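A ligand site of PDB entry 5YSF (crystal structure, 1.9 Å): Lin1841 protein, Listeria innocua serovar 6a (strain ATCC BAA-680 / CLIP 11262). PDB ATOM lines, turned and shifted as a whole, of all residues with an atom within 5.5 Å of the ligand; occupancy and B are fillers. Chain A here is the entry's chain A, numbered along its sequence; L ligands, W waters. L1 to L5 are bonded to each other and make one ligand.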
ATOM      1  N   MET A  17      15.209   5.696 -18.622  1.00  0.00           N
ATOM      2  CA  MET A  17      14.500   6.812 -17.965  1.00  0.00           C
ATOM      3  C   MET A  17      14.245   6.507 -16.493  1.00  0.00           C
ATOM      4  O   MET A  17      13.900   5.419 -16.112  1.00  0.00           O
ATOM      5  CB  MET A  17      13.135   7.089 -18.641  1.00  0.00           C
ATOM      6  CG  MET A  17      13.301   7.730 -19.982  1.00  0.00           C
ATOM      7  SD  MET A  17      13.324   6.459 -21.246  1.00  0.00           S
ATOM      8  CE  MET A  17      14.539   7.161 -22.362  1.00  0.00           C
ATOM      9  N   GLY A  18      14.272   7.567 -15.731  1.00  0.00           N
ATOM     10  CA  GLY A  18      13.727   7.591 -14.408  1.00  0.00           C
ATOM     11  C   GLY A  18      14.295   6.594 -13.472  1.00  0.00           C
ATOM     12  O   GLY A  18      15.436   6.205 -13.614  1.00  0.00           O
ATOM     13  N   ASP A  19      13.459   6.121 -12.557  1.00  0.00           N
ATOM     14  CA  ASP A  19      13.899   5.215 -11.506  1.00  0.00           C
ATOM     15  C   ASP A  19      14.247   3.828 -12.028  1.00  0.00           C
ATOM     16  O   ASP A  19      15.215   3.205 -11.566  1.00  0.00           O
ATOM     17  CB  ASP A  19      12.848   5.086 -10.421  1.00  0.00           C
ATOM     18  CG  ASP A  19      12.820   6.230  -9.540  1.00  0.00           C
ATOM     19  OD1 ASP A  19      13.814   6.985  -9.509  1.00  0.00           O
ATOM     20  OD2 ASP A  19      11.769   6.415  -8.899  1.00  0.00           O
ATOM     21  N   GLU A  20      13.513   3.391 -13.035  1.00  0.00           N
ATOM     22  CA  GLU A  20      13.747   2.029 -13.610  1.00  0.00           C
ATOM     23  C   GLU A  20      15.127   1.968 -14.275  1.00  0.00           C
ATOM     24  O   GLU A  20      15.757   0.895 -14.338  1.00  0.00           O
ATOM     25  CB  GLU A  20      12.601   1.607 -14.586  1.00  0.00           C
ATOM     26  CG  GLU A  20      11.270   1.442 -13.885  1.00  0.00           C
ATOM     27  CD  GLU A  20      10.447   2.752 -13.668  1.00  0.00           C
ATOM     28  OE1 GLU A  20      10.947   3.864 -14.062  1.00  0.00           O
ATOM     29  OE2 GLU A  20       9.307   2.638 -13.130  1.00  0.00           O
ATOM     30  N   TRP A  46      11.742  11.300 -17.556  1.00  0.00           N
ATOM     31  CA  TRP A  46      10.589  11.212 -18.433  1.00  0.00           C
ATOM     32  C   TRP A  46      10.128  12.556 -18.995  1.00  0.00           C
ATOM     33  O   TRP A  46       9.787  12.611 -20.182  1.00  0.00           O
ATOM     34  CB  TRP A  46       9.400  10.497 -17.734  1.00  0.00           C
ATOM     35  CG  TRP A  46       9.577   8.928 -17.752  1.00  0.00           C
ATOM     36  CD1 TRP A  46       9.856   8.085 -16.666  1.00  0.00           C
ATOM     37  CD2 TRP A  46       9.505   8.092 -18.877  1.00  0.00           C
ATOM     38  NE1 TRP A  46       9.967   6.805 -17.081  1.00  0.00           N
ATOM     39  CE2 TRP A  46       9.751   6.760 -18.430  1.00  0.00           C
ATOM     40  CE3 TRP A  46       9.310   8.340 -20.247  1.00  0.00           C
ATOM     41  CZ2 TRP A  46       9.770   5.678 -19.296  1.00  0.00           C
ATOM     42  CZ3 TRP A  46       9.354   7.241 -21.142  1.00  0.00           C
ATOM     43  CH2 TRP A  46       9.595   5.934 -20.659  1.00  0.00           C
ATOM     44  N   GLY A  69       9.071   4.757 -24.049  1.00  0.00           N
ATOM     45  CA  GLY A  69       7.760   4.869 -23.543  1.00  0.00           C
ATOM     46  C   GLY A  69       6.788   4.347 -24.562  1.00  0.00           C
ATOM     47  O   GLY A  69       6.902   4.647 -25.750  1.00  0.00           O
ATOM     48  N   THR A  70       5.847   3.519 -24.109  1.00  0.00           N
ATOM     49  CA  THR A  70       4.966   2.861 -25.054  1.00  0.00           C
ATOM     50  C   THR A  70       4.179   3.810 -25.930  1.00  0.00           C
ATOM     51  O   THR A  70       3.934   3.508 -27.119  1.00  0.00           O
ATOM     52  CB  THR A  70       3.918   1.974 -24.314  1.00  0.00           C
ATOM     53  OG1 THR A  70       3.236   2.758 -23.338  1.00  0.00           O
ATOM     54  CG2 THR A  70       4.614   0.765 -23.681  1.00  0.00           C
ATOM     55  N   THR A  71       3.817   4.951 -25.373  1.00  0.00           N
ATOM     56  CA  THR A  71       2.976   5.913 -26.128  1.00  0.00           C
ATOM     57  C   THR A  71       3.717   6.593 -27.270  1.00  0.00           C
ATOM     58  O   THR A  71       3.066   7.194 -28.128  1.00  0.00           O
ATOM     59  CB  THR A  71       2.399   7.031 -25.220  1.00  0.00           C
ATOM     60  OG1 THR A  71       3.419   7.864 -24.716  1.00  0.00           O
ATOM     61  CG2 THR A  71       1.570   6.417 -24.054  1.00  0.00           C
ATOM     62  N   TRP A  72       5.046   6.520 -27.230  1.00  0.00           N
ATOM     63  CA  TRP A  72       5.903   7.114 -28.252  1.00  0.00           C
ATOM     64  C   TRP A  72       6.350   6.104 -29.328  1.00  0.00           C
ATOM     65  O   TRP A  72       7.000   6.493 -30.296  1.00  0.00           O
ATOM     66  CB  TRP A  72       7.125   7.796 -27.611  1.00  0.00           C
ATOM     67  CG  TRP A  72       6.767   8.903 -26.654  1.00  0.00           C
ATOM     68  CD1 TRP A  72       5.564   9.664 -26.606  1.00  0.00           C
ATOM     69  CD2 TRP A  72       7.523   9.325 -25.540  1.00  0.00           C
ATOM     70  NE1 TRP A  72       5.624  10.525 -25.552  1.00  0.00           N
ATOM     71  CE2 TRP A  72       6.815  10.325 -24.881  1.00  0.00           C
ATOM     72  CE3 TRP A  72       8.806   8.966 -25.057  1.00  0.00           C
ATOM     73  CZ2 TRP A  72       7.310  10.977 -23.738  1.00  0.00           C
ATOM     74  CZ3 TRP A  72       9.312   9.604 -23.927  1.00  0.00           C
ATOM     75  CH2 TRP A  72       8.554  10.595 -23.259  1.00  0.00           C
ATOM     76  N   TYR A 120       8.609  -3.456 -19.169  1.00  0.00           N
ATOM     77  CA  TYR A 120       7.608  -3.467 -18.087  1.00  0.00           C
ATOM     78  C   TYR A 120       6.273  -2.807 -18.594  1.00  0.00           C
ATOM     79  O   TYR A 120       6.276  -2.092 -19.606  1.00  0.00           O
ATOM     80  CB  TYR A 120       8.180  -2.832 -16.801  1.00  0.00           C
ATOM     81  CG  TYR A 120       8.323  -1.333 -16.912  1.00  0.00           C
ATOM     82  CD1 TYR A 120       7.292  -0.486 -16.645  1.00  0.00           C
ATOM     83  CD2 TYR A 120       9.536  -0.756 -17.306  1.00  0.00           C
ATOM     84  CE1 TYR A 120       7.412   0.925 -16.782  1.00  0.00           C
ATOM     85  CE2 TYR A 120       9.703   0.606 -17.421  1.00  0.00           C
ATOM     86  CZ  TYR A 120       8.652   1.466 -17.182  1.00  0.00           C
ATOM     87  OH  TYR A 120       8.894   2.779 -17.344  1.00  0.00           O
ATOM     88  N   GLU A 122       2.459  -0.938 -17.103  1.00  0.00           N
ATOM     89  CA  GLU A 122       1.833  -0.286 -15.979  1.00  0.00           C
ATOM     90  C   GLU A 122       0.397   0.034 -16.357  1.00  0.00           C
ATOM     91  O   GLU A 122      -0.020   0.067 -17.547  1.00  0.00           O
ATOM     92  CB  GLU A 122       2.556   0.973 -15.497  1.00  0.00           C
ATOM     93  CG  GLU A 122       2.960   1.996 -16.559  1.00  0.00           C
ATOM     94  CD  GLU A 122       1.862   3.031 -16.874  1.00  0.00           C
ATOM     95  OE1 GLU A 122       0.799   2.929 -16.248  1.00  0.00           O
ATOM     96  OE2 GLU A 122       2.082   3.915 -17.716  1.00  0.00           O
ATOM     97  N   ARG A 124      -3.026   2.531 -14.493  1.00  0.00           N
ATOM     98  CA  ARG A 124      -3.350   3.484 -13.434  1.00  0.00           C
ATOM     99  C   ARG A 124      -4.526   3.031 -12.594  1.00  0.00           C
ATOM    100  O   ARG A 124      -5.582   2.637 -13.092  1.00  0.00           O
ATOM    101  CB  ARG A 124      -3.573   4.869 -14.010  1.00  0.00           C
ATOM    102  CG  ARG A 124      -2.510   5.290 -15.008  1.00  0.00           C
ATOM    103  CD  ARG A 124      -1.074   5.217 -14.381  1.00  0.00           C
ATOM    104  NE  ARG A 124      -0.107   5.440 -15.459  1.00  0.00           N
ATOM    105  CZ  ARG A 124       0.405   6.574 -15.875  1.00  0.00           C
ATOM    106  NH1 ARG A 124       0.071   7.752 -15.353  1.00  0.00           N
ATOM    107  NH2 ARG A 124       1.265   6.534 -16.888  1.00  0.00           N
ATOM    108  N   ALA A 166      -6.610  14.466  -6.562  1.00  0.00           N
ATOM    109  CA  ALA A 166      -5.639  15.214  -7.356  1.00  0.00           C
ATOM    110  C   ALA A 166      -5.928  14.929  -8.838  1.00  0.00           C
ATOM    111  O   ALA A 166      -6.175  13.786  -9.196  1.00  0.00           O
ATOM    112  CB  ALA A 166      -4.260  14.705  -7.038  1.00  0.00           C
ATOM    113  N   ASP A 168      -3.556  15.592 -12.096  1.00  0.00           N
ATOM    114  CA  ASP A 168      -2.213  16.017 -12.443  1.00  0.00           C
ATOM    115  C   ASP A 168      -2.306  16.704 -13.826  1.00  0.00           C
ATOM    116  O   ASP A 168      -2.576  16.071 -14.868  1.00  0.00           O
ATOM    117  CB  ASP A 168      -1.281  14.807 -12.480  1.00  0.00           C
ATOM    118  CG  ASP A 168       0.116  15.136 -12.890  1.00  0.00           C
ATOM    119  OD1 ASP A 168       0.403  16.280 -13.366  1.00  0.00           O
ATOM    120  OD2 ASP A 168       0.943  14.160 -12.793  1.00  0.00           O
ATOM    121  N   ASN A 170      -0.141  17.705 -15.842  1.00  0.00           N
ATOM    122  CA  ASN A 170       0.919  17.278 -16.769  1.00  0.00           C
ATOM    123  C   ASN A 170       0.820  15.784 -17.153  1.00  0.00           C
ATOM    124  O   ASN A 170       1.609  15.354 -17.975  1.00  0.00           O
ATOM    125  CB  ASN A 170       2.305  17.509 -16.190  1.00  0.00           C
ATOM    126  CG  ASN A 170       2.538  18.956 -15.787  1.00  0.00           C
ATOM    127  OD1 ASN A 170       3.268  19.161 -14.813  1.00  0.00           O
ATOM    128  ND2 ASN A 170       1.978  19.914 -16.476  1.00  0.00           N
ATOM    129  N   GLU A 171      -0.178  15.073 -16.619  1.00  0.00           N
ATOM    130  CA  GLU A 171      -0.354  13.689 -16.928  1.00  0.00           C
ATOM    131  C   GLU A 171      -1.096  13.498 -18.251  1.00  0.00           C
ATOM    132  O   GLU A 171      -2.298  13.791 -18.367  1.00  0.00           O
ATOM    133  CB  GLU A 171      -1.127  13.026 -15.769  1.00  0.00           C
ATOM    134  CG  GLU A 171      -1.431  11.582 -15.977  1.00  0.00           C
ATOM    135  CD  GLU A 171      -0.247  10.736 -16.478  1.00  0.00           C
ATOM    136  OE1 GLU A 171       0.741  10.643 -15.757  1.00  0.00           O
ATOM    137  OE2 GLU A 171      -0.346  10.167 -17.617  1.00  0.00           O
ATOM    138  N   GLN A 172      -0.422  12.936 -19.229  1.00  0.00           N
ATOM    139  CA  GLN A 172      -0.970  12.750 -20.569  1.00  0.00           C
ATOM    140  C   GLN A 172      -2.240  11.868 -20.596  1.00  0.00           C
ATOM    141  O   GLN A 172      -3.087  12.035 -21.432  1.00  0.00           O
ATOM    142  CB  GLN A 172       0.089  12.139 -21.527  1.00  0.00           C
ATOM    143  CG  GLN A 172       1.298  13.023 -21.738  1.00  0.00           C
ATOM    144  CD  GLN A 172       2.464  12.664 -20.833  1.00  0.00           C
ATOM    145  OE1 GLN A 172       2.252  12.224 -19.713  1.00  0.00           O
ATOM    146  NE2 GLN A 172       3.702  12.879 -21.311  1.00  0.00           N
ATOM    147  N   PHE A 238      -5.720   9.965  -5.182  1.00  0.00           N
ATOM    148  CA  PHE A 238      -5.074  10.289  -6.452  1.00  0.00           C
ATOM    149  C   PHE A 238      -4.978   9.054  -7.324  1.00  0.00           C
ATOM    150  O   PHE A 238      -5.257   7.972  -6.873  1.00  0.00           O
ATOM    151  CB  PHE A 238      -3.701  10.981  -6.225  1.00  0.00           C
ATOM    152  CG  PHE A 238      -2.612  10.087  -5.662  1.00  0.00           C
ATOM    153  CD1 PHE A 238      -1.816   9.338  -6.503  1.00  0.00           C
ATOM    154  CD2 PHE A 238      -2.406   9.952  -4.245  1.00  0.00           C
ATOM    155  CE1 PHE A 238      -0.809   8.524  -6.014  1.00  0.00           C
ATOM    156  CE2 PHE A 238      -1.413   9.145  -3.788  1.00  0.00           C
ATOM    157  CZ  PHE A 238      -0.615   8.446  -4.652  1.00  0.00           C
ATOM    158  N   MET A 239      -4.544   9.234  -8.566  1.00  0.00           N
ATOM    159  CA  MET A 239      -4.391   8.156  -9.515  1.00  0.00           C
ATOM    160  C   MET A 239      -2.927   8.065  -9.914  1.00  0.00           C
ATOM    161  O   MET A 239      -2.244   9.077 -10.190  1.00  0.00           O
ATOM    162  CB  MET A 239      -5.186   8.471 -10.812  1.00  0.00           C
ATOM    163  CG  MET A 239      -6.647   8.256 -10.594  1.00  0.00           C
ATOM    164  SD  MET A 239      -7.572   8.970 -11.998  1.00  0.00           S
ATOM    165  CE  MET A 239      -6.884   8.084 -13.455  1.00  0.00           C
ATOM    166  N   SER A 240      -2.394   6.862  -9.888  1.00  0.00           N
ATOM    167  CA  SER A 240      -1.058   6.643 -10.451  1.00  0.00           C
ATOM    168  C   SER A 240      -0.807   5.164 -10.755  1.00  0.00           C
ATOM    169  O   SER A 240      -1.699   4.311 -10.636  1.00  0.00           O
ATOM    170  CB  SER A 240      -0.009   7.136  -9.447  1.00  0.00           C
ATOM    171  OG  SER A 240       1.190   7.427 -10.124  1.00  0.00           O
ATOM    172  N   GLY A 241       0.452   4.871 -11.030  1.00  0.00           N
ATOM    173  CA  GLY A 241       0.913   3.547 -11.353  1.00  0.00           C
ATOM    174  C   GLY A 241       1.781   2.947 -10.247  1.00  0.00           C
ATOM    175  O   GLY A 241       1.871   3.496  -9.152  1.00  0.00           O
ATOM    176  N   TRP A 243       4.940   2.596  -9.620  1.00  0.00           N
ATOM    177  CA  TRP A 243       6.022   3.393  -9.030  1.00  0.00           C
ATOM    178  C   TRP A 243       5.630   4.135  -7.742  1.00  0.00           C
ATOM    179  O   TRP A 243       6.452   4.242  -6.873  1.00  0.00           O
ATOM    180  CB  TRP A 243       6.665   4.323 -10.064  1.00  0.00           C
ATOM    181  CG  TRP A 243       5.734   5.399 -10.484  1.00  0.00           C
ATOM    182  CD1 TRP A 243       5.667   6.681  -9.988  1.00  0.00           C
ATOM    183  CD2 TRP A 243       4.789   5.317 -11.567  1.00  0.00           C
ATOM    184  NE1 TRP A 243       4.694   7.390 -10.736  1.00  0.00           N
ATOM    185  CE2 TRP A 243       4.144   6.541 -11.664  1.00  0.00           C
ATOM    186  CE3 TRP A 243       4.465   4.302 -12.466  1.00  0.00           C
ATOM    187  CZ2 TRP A 243       3.208   6.811 -12.633  1.00  0.00           C
ATOM    188  CZ3 TRP A 243       3.452   4.597 -13.489  1.00  0.00           C
ATOM    189  CH2 TRP A 243       2.872   5.834 -13.523  1.00  0.00           C
ATOM    190  N   MET A 244       4.357   4.545  -7.588  1.00  0.00           N
ATOM    191  CA  MET A 244       3.844   5.222  -6.393  1.00  0.00           C
ATOM    192  C   MET A 244       3.605   4.296  -5.211  1.00  0.00           C
ATOM    193  O   MET A 244       3.717   4.722  -4.093  1.00  0.00           O
ATOM    194  CB  MET A 244       2.537   6.035  -6.670  1.00  0.00           C
ATOM    195  CG  MET A 244       2.881   7.217  -7.600  1.00  0.00           C
ATOM    196  SD  MET A 244       4.165   8.401  -7.020  1.00  0.00           S
ATOM    197  CE  MET A 244       3.423   8.417  -5.347  1.00  0.00           C
ATOM    198  N   LEU A 274      -3.070   1.420 -20.426  1.00  0.00           N
ATOM    199  CA  LEU A 274      -1.962   0.489 -20.435  1.00  0.00           C
ATOM    200  C   LEU A 274      -0.749   1.206 -20.972  1.00  0.00           C
ATOM    201  O   LEU A 274      -0.730   1.724 -22.135  1.00  0.00           O
ATOM    202  CB  LEU A 274      -2.216  -0.734 -21.322  1.00  0.00           C
ATOM    203  CG  LEU A 274      -1.113  -1.788 -21.239  1.00  0.00           C
ATOM    204  CD1 LEU A 274      -1.031  -2.433 -19.872  1.00  0.00           C
ATOM    205  CD2 LEU A 274      -1.416  -2.900 -22.239  1.00  0.00           C
ATOM    206  N   GLY A 275       0.280   1.230 -20.147  1.00  0.00           N
ATOM    207  CA  GLY A 275       1.538   1.798 -20.564  1.00  0.00           C
ATOM    208  C   GLY A 275       2.741   0.957 -20.173  1.00  0.00           C
ATOM    209  O   GLY A 275       2.635  -0.257 -19.995  1.00  0.00           O
ATOM    210  N   GLY A 276       3.859   1.667 -20.000  1.00  0.00           N
ATOM    211  CA  GLY A 276       5.107   1.117 -19.579  1.00  0.00           C
ATOM    212  C   GLY A 276       6.179   1.489 -20.607  1.00  0.00           C
ATOM    213  O   GLY A 276       6.142   2.571 -21.234  1.00  0.00           O
ATOM    214  N   ALA A 277       7.182   0.603 -20.720  1.00  0.00           N
ATOM    215  CA  ALA A 277       8.248   0.799 -21.652  1.00  0.00           C
ATOM    216  C   ALA A 277       8.662  -0.507 -22.345  1.00  0.00           C
ATOM    217  O   ALA A 277       8.503  -1.578 -21.794  1.00  0.00           O
ATOM    218  CB  ALA A 277       9.415   1.454 -20.992  1.00  0.00           C
ATOM    219  N   GLU A 352       1.952  12.314 -28.537  1.00  0.00           N
ATOM    220  CA  GLU A 352       2.495  13.235 -27.530  1.00  0.00           C
ATOM    221  C   GLU A 352       2.094  14.676 -27.833  1.00  0.00           C
ATOM    222  O   GLU A 352       1.771  15.430 -26.927  1.00  0.00           O
ATOM    223  CB  GLU A 352       4.001  13.124 -27.399  1.00  0.00           C
ATOM    224  CG  GLU A 352       4.609  13.868 -26.204  1.00  0.00           C
ATOM    225  CD  GLU A 352       4.032  13.349 -24.843  1.00  0.00           C
ATOM    226  OE1 GLU A 352       3.509  12.227 -24.794  1.00  0.00           O
ATOM    227  OE2 GLU A 352       4.144  14.060 -23.847  1.00  0.00           O
HETATM  228  C1  LIG L   1       4.116  11.715 -10.429  1.00  0.00           C
HETATM  229  C2  LIG L   1       3.045  10.955 -11.228  1.00  0.00           C
HETATM  230  C3  LIG L   1       1.823  10.699 -10.318  1.00  0.00           C
HETATM  231  C4  LIG L   1       1.233  12.023  -9.789  1.00  0.00           C
HETATM  232  C5  LIG L   1       0.011  11.810  -8.852  1.00  0.00           C
HETATM  233  C6  LIG L   1       3.445  12.998  -9.894  1.00  0.00           C
HETATM  234  O1  LIG L   1       4.354  13.733  -9.070  1.00  0.00           O
HETATM  235  O2  LIG L   1       5.271  11.993 -11.251  1.00  0.00           O
HETATM  236  O3  LIG L   1       3.572   9.712 -11.722  1.00  0.00           O
HETATM  237  O4  LIG L   1       0.880   9.902 -11.048  1.00  0.00           O
HETATM  238  O5  LIG L   1       2.299  12.716  -9.077  1.00  0.00           O
HETATM  239  O6  LIG L   1      -1.130  12.672  -9.146  1.00  0.00           O
HETATM  240  C1  LG2 L   2       6.953  10.820 -12.591  1.00  0.00           C
HETATM  241  C2  LG2 L   2       8.158   9.893 -12.466  1.00  0.00           C
HETATM  242  C3  LG2 L   2       9.206  10.550 -11.558  1.00  0.00           C
HETATM  243  C4  LG2 L   2       8.602  11.043 -10.255  1.00  0.00           C
HETATM  244  C5  LG2 L   2       9.578  12.011  -9.588  1.00  0.00           C
HETATM  245  C6  LG2 L   2       6.390  11.102 -11.184  1.00  0.00           C
HETATM  246  O1  LG2 L   2       5.972  10.198 -13.405  1.00  0.00           O
HETATM  247  O2  LG2 L   2       8.792   9.639 -13.718  1.00  0.00           O
HETATM  248  O3  LG2 L   2      10.179   9.607 -11.168  1.00  0.00           O
HETATM  249  O4  LG2 L   2       7.398  11.785 -10.452  1.00  0.00           O
HETATM  250  O5  LG2 L   2       9.089  12.220  -8.277  1.00  0.00           O
HETATM  251  C1  LG3 L   3       5.253   9.859 -15.656  1.00  0.00           C
HETATM  252  C2  LG3 L   3       4.990  10.633 -16.927  1.00  0.00           C
HETATM  253  C3  LG3 L   3       3.980  11.735 -16.714  1.00  0.00           C
HETATM  254  C4  LG3 L   3       4.303  12.572 -15.492  1.00  0.00           C
HETATM  255  C5  LG3 L   3       3.151  13.533 -15.239  1.00  0.00           C
HETATM  256  C6  LG3 L   3       5.661  10.856 -14.603  1.00  0.00           C
HETATM  257  O1  LG3 L   3       6.297   8.937 -15.965  1.00  0.00           O
HETATM  258  O2  LG3 L   3       4.552   9.820 -17.989  1.00  0.00           O
HETATM  259  O3  LG3 L   3       4.047  12.547 -17.871  1.00  0.00           O
HETATM  260  O4  LG3 L   3       4.555  11.735 -14.344  1.00  0.00           O
HETATM  261  O5  LG3 L   3       3.266  14.191 -13.993  1.00  0.00           O
HETATM  262  C1  LG4 L   4       6.374   6.572 -16.627  1.00  0.00           C
HETATM  263  C2  LG4 L   4       6.326   5.163 -16.021  1.00  0.00           C
HETATM  264  C3  LG4 L   4       7.445   5.018 -14.948  1.00  0.00           C
HETATM  265  C4  LG4 L   4       7.378   6.171 -13.936  1.00  0.00           C
HETATM  266  C5  LG4 L   4       8.513   6.145 -12.904  1.00  0.00           C
HETATM  267  C6  LG4 L   4       6.250   7.604 -15.506  1.00  0.00           C
HETATM  268  O1  LG4 L   4       5.234   6.758 -17.474  1.00  0.00           O
HETATM  269  O2  LG4 L   4       6.540   4.132 -16.997  1.00  0.00           O
HETATM  270  O3  LG4 L   4       7.238   3.765 -14.303  1.00  0.00           O
HETATM  271  O4  LG4 L   4       7.316   7.457 -14.580  1.00  0.00           O
HETATM  272  O5  LG4 L   4       9.783   6.150 -13.559  1.00  0.00           O
HETATM  273  C1  LG5 L   5       4.372   5.577 -19.306  1.00  0.00           C
HETATM  274  C2  LG5 L   5       4.466   5.329 -20.810  1.00  0.00           C
HETATM  275  C3  LG5 L   5       4.600   6.640 -21.535  1.00  0.00           C
HETATM  276  C4  LG5 L   5       5.699   7.506 -20.910  1.00  0.00           C
HETATM  277  C5  LG5 L   5       5.790   8.876 -21.539  1.00  0.00           C
HETATM  278  C6  LG5 L   5       5.504   6.442 -18.832  1.00  0.00           C
HETATM  279  O1  LG5 L   5       4.429   4.288 -18.691  1.00  0.00           O
HETATM  280  O2  LG5 L   5       3.356   4.516 -21.198  1.00  0.00           O
HETATM  281  O3  LG5 L   5       4.919   6.396 -22.898  1.00  0.00           O
HETATM  282  O4  LG5 L   5       5.550   7.672 -19.477  1.00  0.00           O
HETATM  283  O5  LG5 L   5       4.617   9.656 -21.165  1.00  0.00           O
HETATM  284  O   HOH W   1       1.872  13.975  -6.111  1.00  0.00           O
HETATM  285  O   HOH W   2       0.217  11.367 -13.052  1.00  0.00           O
HETATM  286  O   HOH W   3       1.927   8.950 -18.472  1.00  0.00           O
HETATM  287  O   HOH W   4       6.525  12.130 -20.180  1.00  0.00           O
HETATM  288  O   HOH W   5       2.904  10.017 -23.190  1.00  0.00           O
HETATM  289  O   HOH W   6       0.790   5.726 -20.823  1.00  0.00           O
HETATM  290  O   HOH W   7       5.937   1.680 -13.350  1.00  0.00           O
HETATM  291  O   HOH W   8       6.546  13.865 -18.111  1.00  0.00           O
HETATM  292  O   HOH W   9      -3.929  11.958  -9.575  1.00  0.00           O
HETATM  293  O   HOH W  10      11.215  10.801 -14.685  1.00  0.00           O
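The side-chain carboxylate of Glu 122 is in hydrogen-bond range of an oxygen (O1) of LG5 L5, at 2.6 Å. The side-chain amide oxygen (OE1) of Gln 172 is in hydrogen-bond range of an oxygen (O3) of LG3 L3 (2.6 Å). The side-chain carboxylate (OE1) of Glu 20 is in hydrogen-bond range of an oxygen (O5) of LG4 L4, 2.6 Å away. An oxygen (O5) of LG3 L3 is in hydrogen-bond range of the side-chain carboxylate (OD2) of Asp 168, at 2.6 Å. OG of Ser 240 sits at hydrogen-bond distance from O4 of LIG L1 (2.7 Å). The side-chain hydroxyl (OH) of Tyr 120 is in hydrogen-bond range of an oxygen (O2) of LG4 L4. NE1 of Trp 243 lies within hydrogen-bond range of O3 of LIG L1 (2.8 Å). The backbone NH (N) of Thr 70 is in hydrogen-bond range of an oxygen (O3) of LG5 L5 (3.3 Å). An oxygen (O2) of LG5 L5 sits at hydrogen-bond distance from the side-chain hydroxyl of Thr 70 (2.8 Å). An oxygen (O3) of LG5 L5 is in hydrogen-bond range of the backbone NH (N) of Thr 71 (3.1 Å). An oxygen (O3) of LG5 L5 lies within hydrogen-bond range of the side-chain hydroxyl of Thr 71, at 2.8 Å. N of Gly 276 sits at hydrogen-bond distance from O1 of LG5 L5, at 3.0 Å. O of Gly 276 lies close to O2 of LG5 L5 (3.4 Å). O of Met 239 sits at hydrogen-bond distance from O4 of LIG L1 (3.3 Å).
N of Gly 275 sits at hydrogen-bond distance from O of Glu 122, 2.9 Å away. The side-chain carboxylate (OE1) of Glu 122 is in salt-bridge range of the guanidinium group (NE) of Arg 124 (2.8 Å). The side-chain amide nitrogen (NE2) of Gln 172 sits at hydrogen-bond distance from the side-chain carboxylate (OE2) of Glu 352, 2.8 Å away. The side-chain carboxylate (OD1) of Asp 168 sits at hydrogen-bond distance from the backbone NH (N) of Asn 170, at 2.9 Å. The backbone carbonyl oxygen of Tyr 120 sits at hydrogen-bond distance from the backbone NH of Ala 277, at 3.1 Å. The backbone NH (N) of Thr 70 sits at hydrogen-bond distance from the backbone carbonyl oxygen (O) of Gly 276, 3.0 Å away. The indole nitrogen of Trp 72 is in hydrogen-bond range of the side-chain carboxylate of Glu 352, at 2.8 Å. The guanidinium group (NH1) of Arg 124 is in salt-bridge range of the side-chain carboxylate (OE1) of Glu 171.
N of Asp 19 touches O5 of LG4 L4, 3.8 Å away. CD1 of Trp 46 touches O4 of LG4 L4, at 3.3 Å. C of Gly 69 touches O3 of LG5 L5, 3.2 Å away. Trp 72 touches the ligand. O of Asn 170 touches C5 of LG3 L3, at 3.6 Å. OE1 of Glu 171 touches C3 of LG3 L3, at 3.5 Å. CD1 of Phe 238 touches C5 of LIG L1, 3.9 Å away. Gly 275 touches the ligand. Hydrophobic or aromatic side chains that line the ligand: Trp 46, Trp 72, Tyr 120, Phe 238 and Trp 243. The nearest printed residue that does not touch the ligand is Arg 124 (4.02 Å).
Water W2 lies within hydrogen-bond range of O4 of LIG L1, OE1 of Glu 171 and OD2 of Asp 168. Water W5 lies within hydrogen-bond range of an oxygen (O5) of LG5 L5 (2.7 Å), the side-chain hydroxyl (OG1) of Thr 71 (2.7 Å) and the side-chain carboxylate (OE1) of Glu 352 (2.8 Å). Water W3 lies within hydrogen-bond range of OE2 of Glu 171 (2.7 Å), O2 of LG3 L3 (2.8 Å) and NH2 of Arg 124 (3.0 Å). Water W10 lies within hydrogen-bond range of an oxygen (O2) of LG2 L2 (2.9 Å) and the backbone NH of Trp 46 (3.0 Å). Water W9 lies within hydrogen-bond range of the backbone carbonyl oxygen (O) of Ala 166 (2.9 Å), an oxygen (O6) of LIG L1 (2.9 Å) and the backbone NH (N) of Met 239 (3.0 Å). Water W4 lies within hydrogen-bond range of the side-chain amide nitrogen (NE2) of Gln 172 (3.1 Å), an oxygen (O5) of LG5 L5 (3.3 Å) and the backbone carbonyl oxygen (O) of Trp 46 (3.3 Å).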
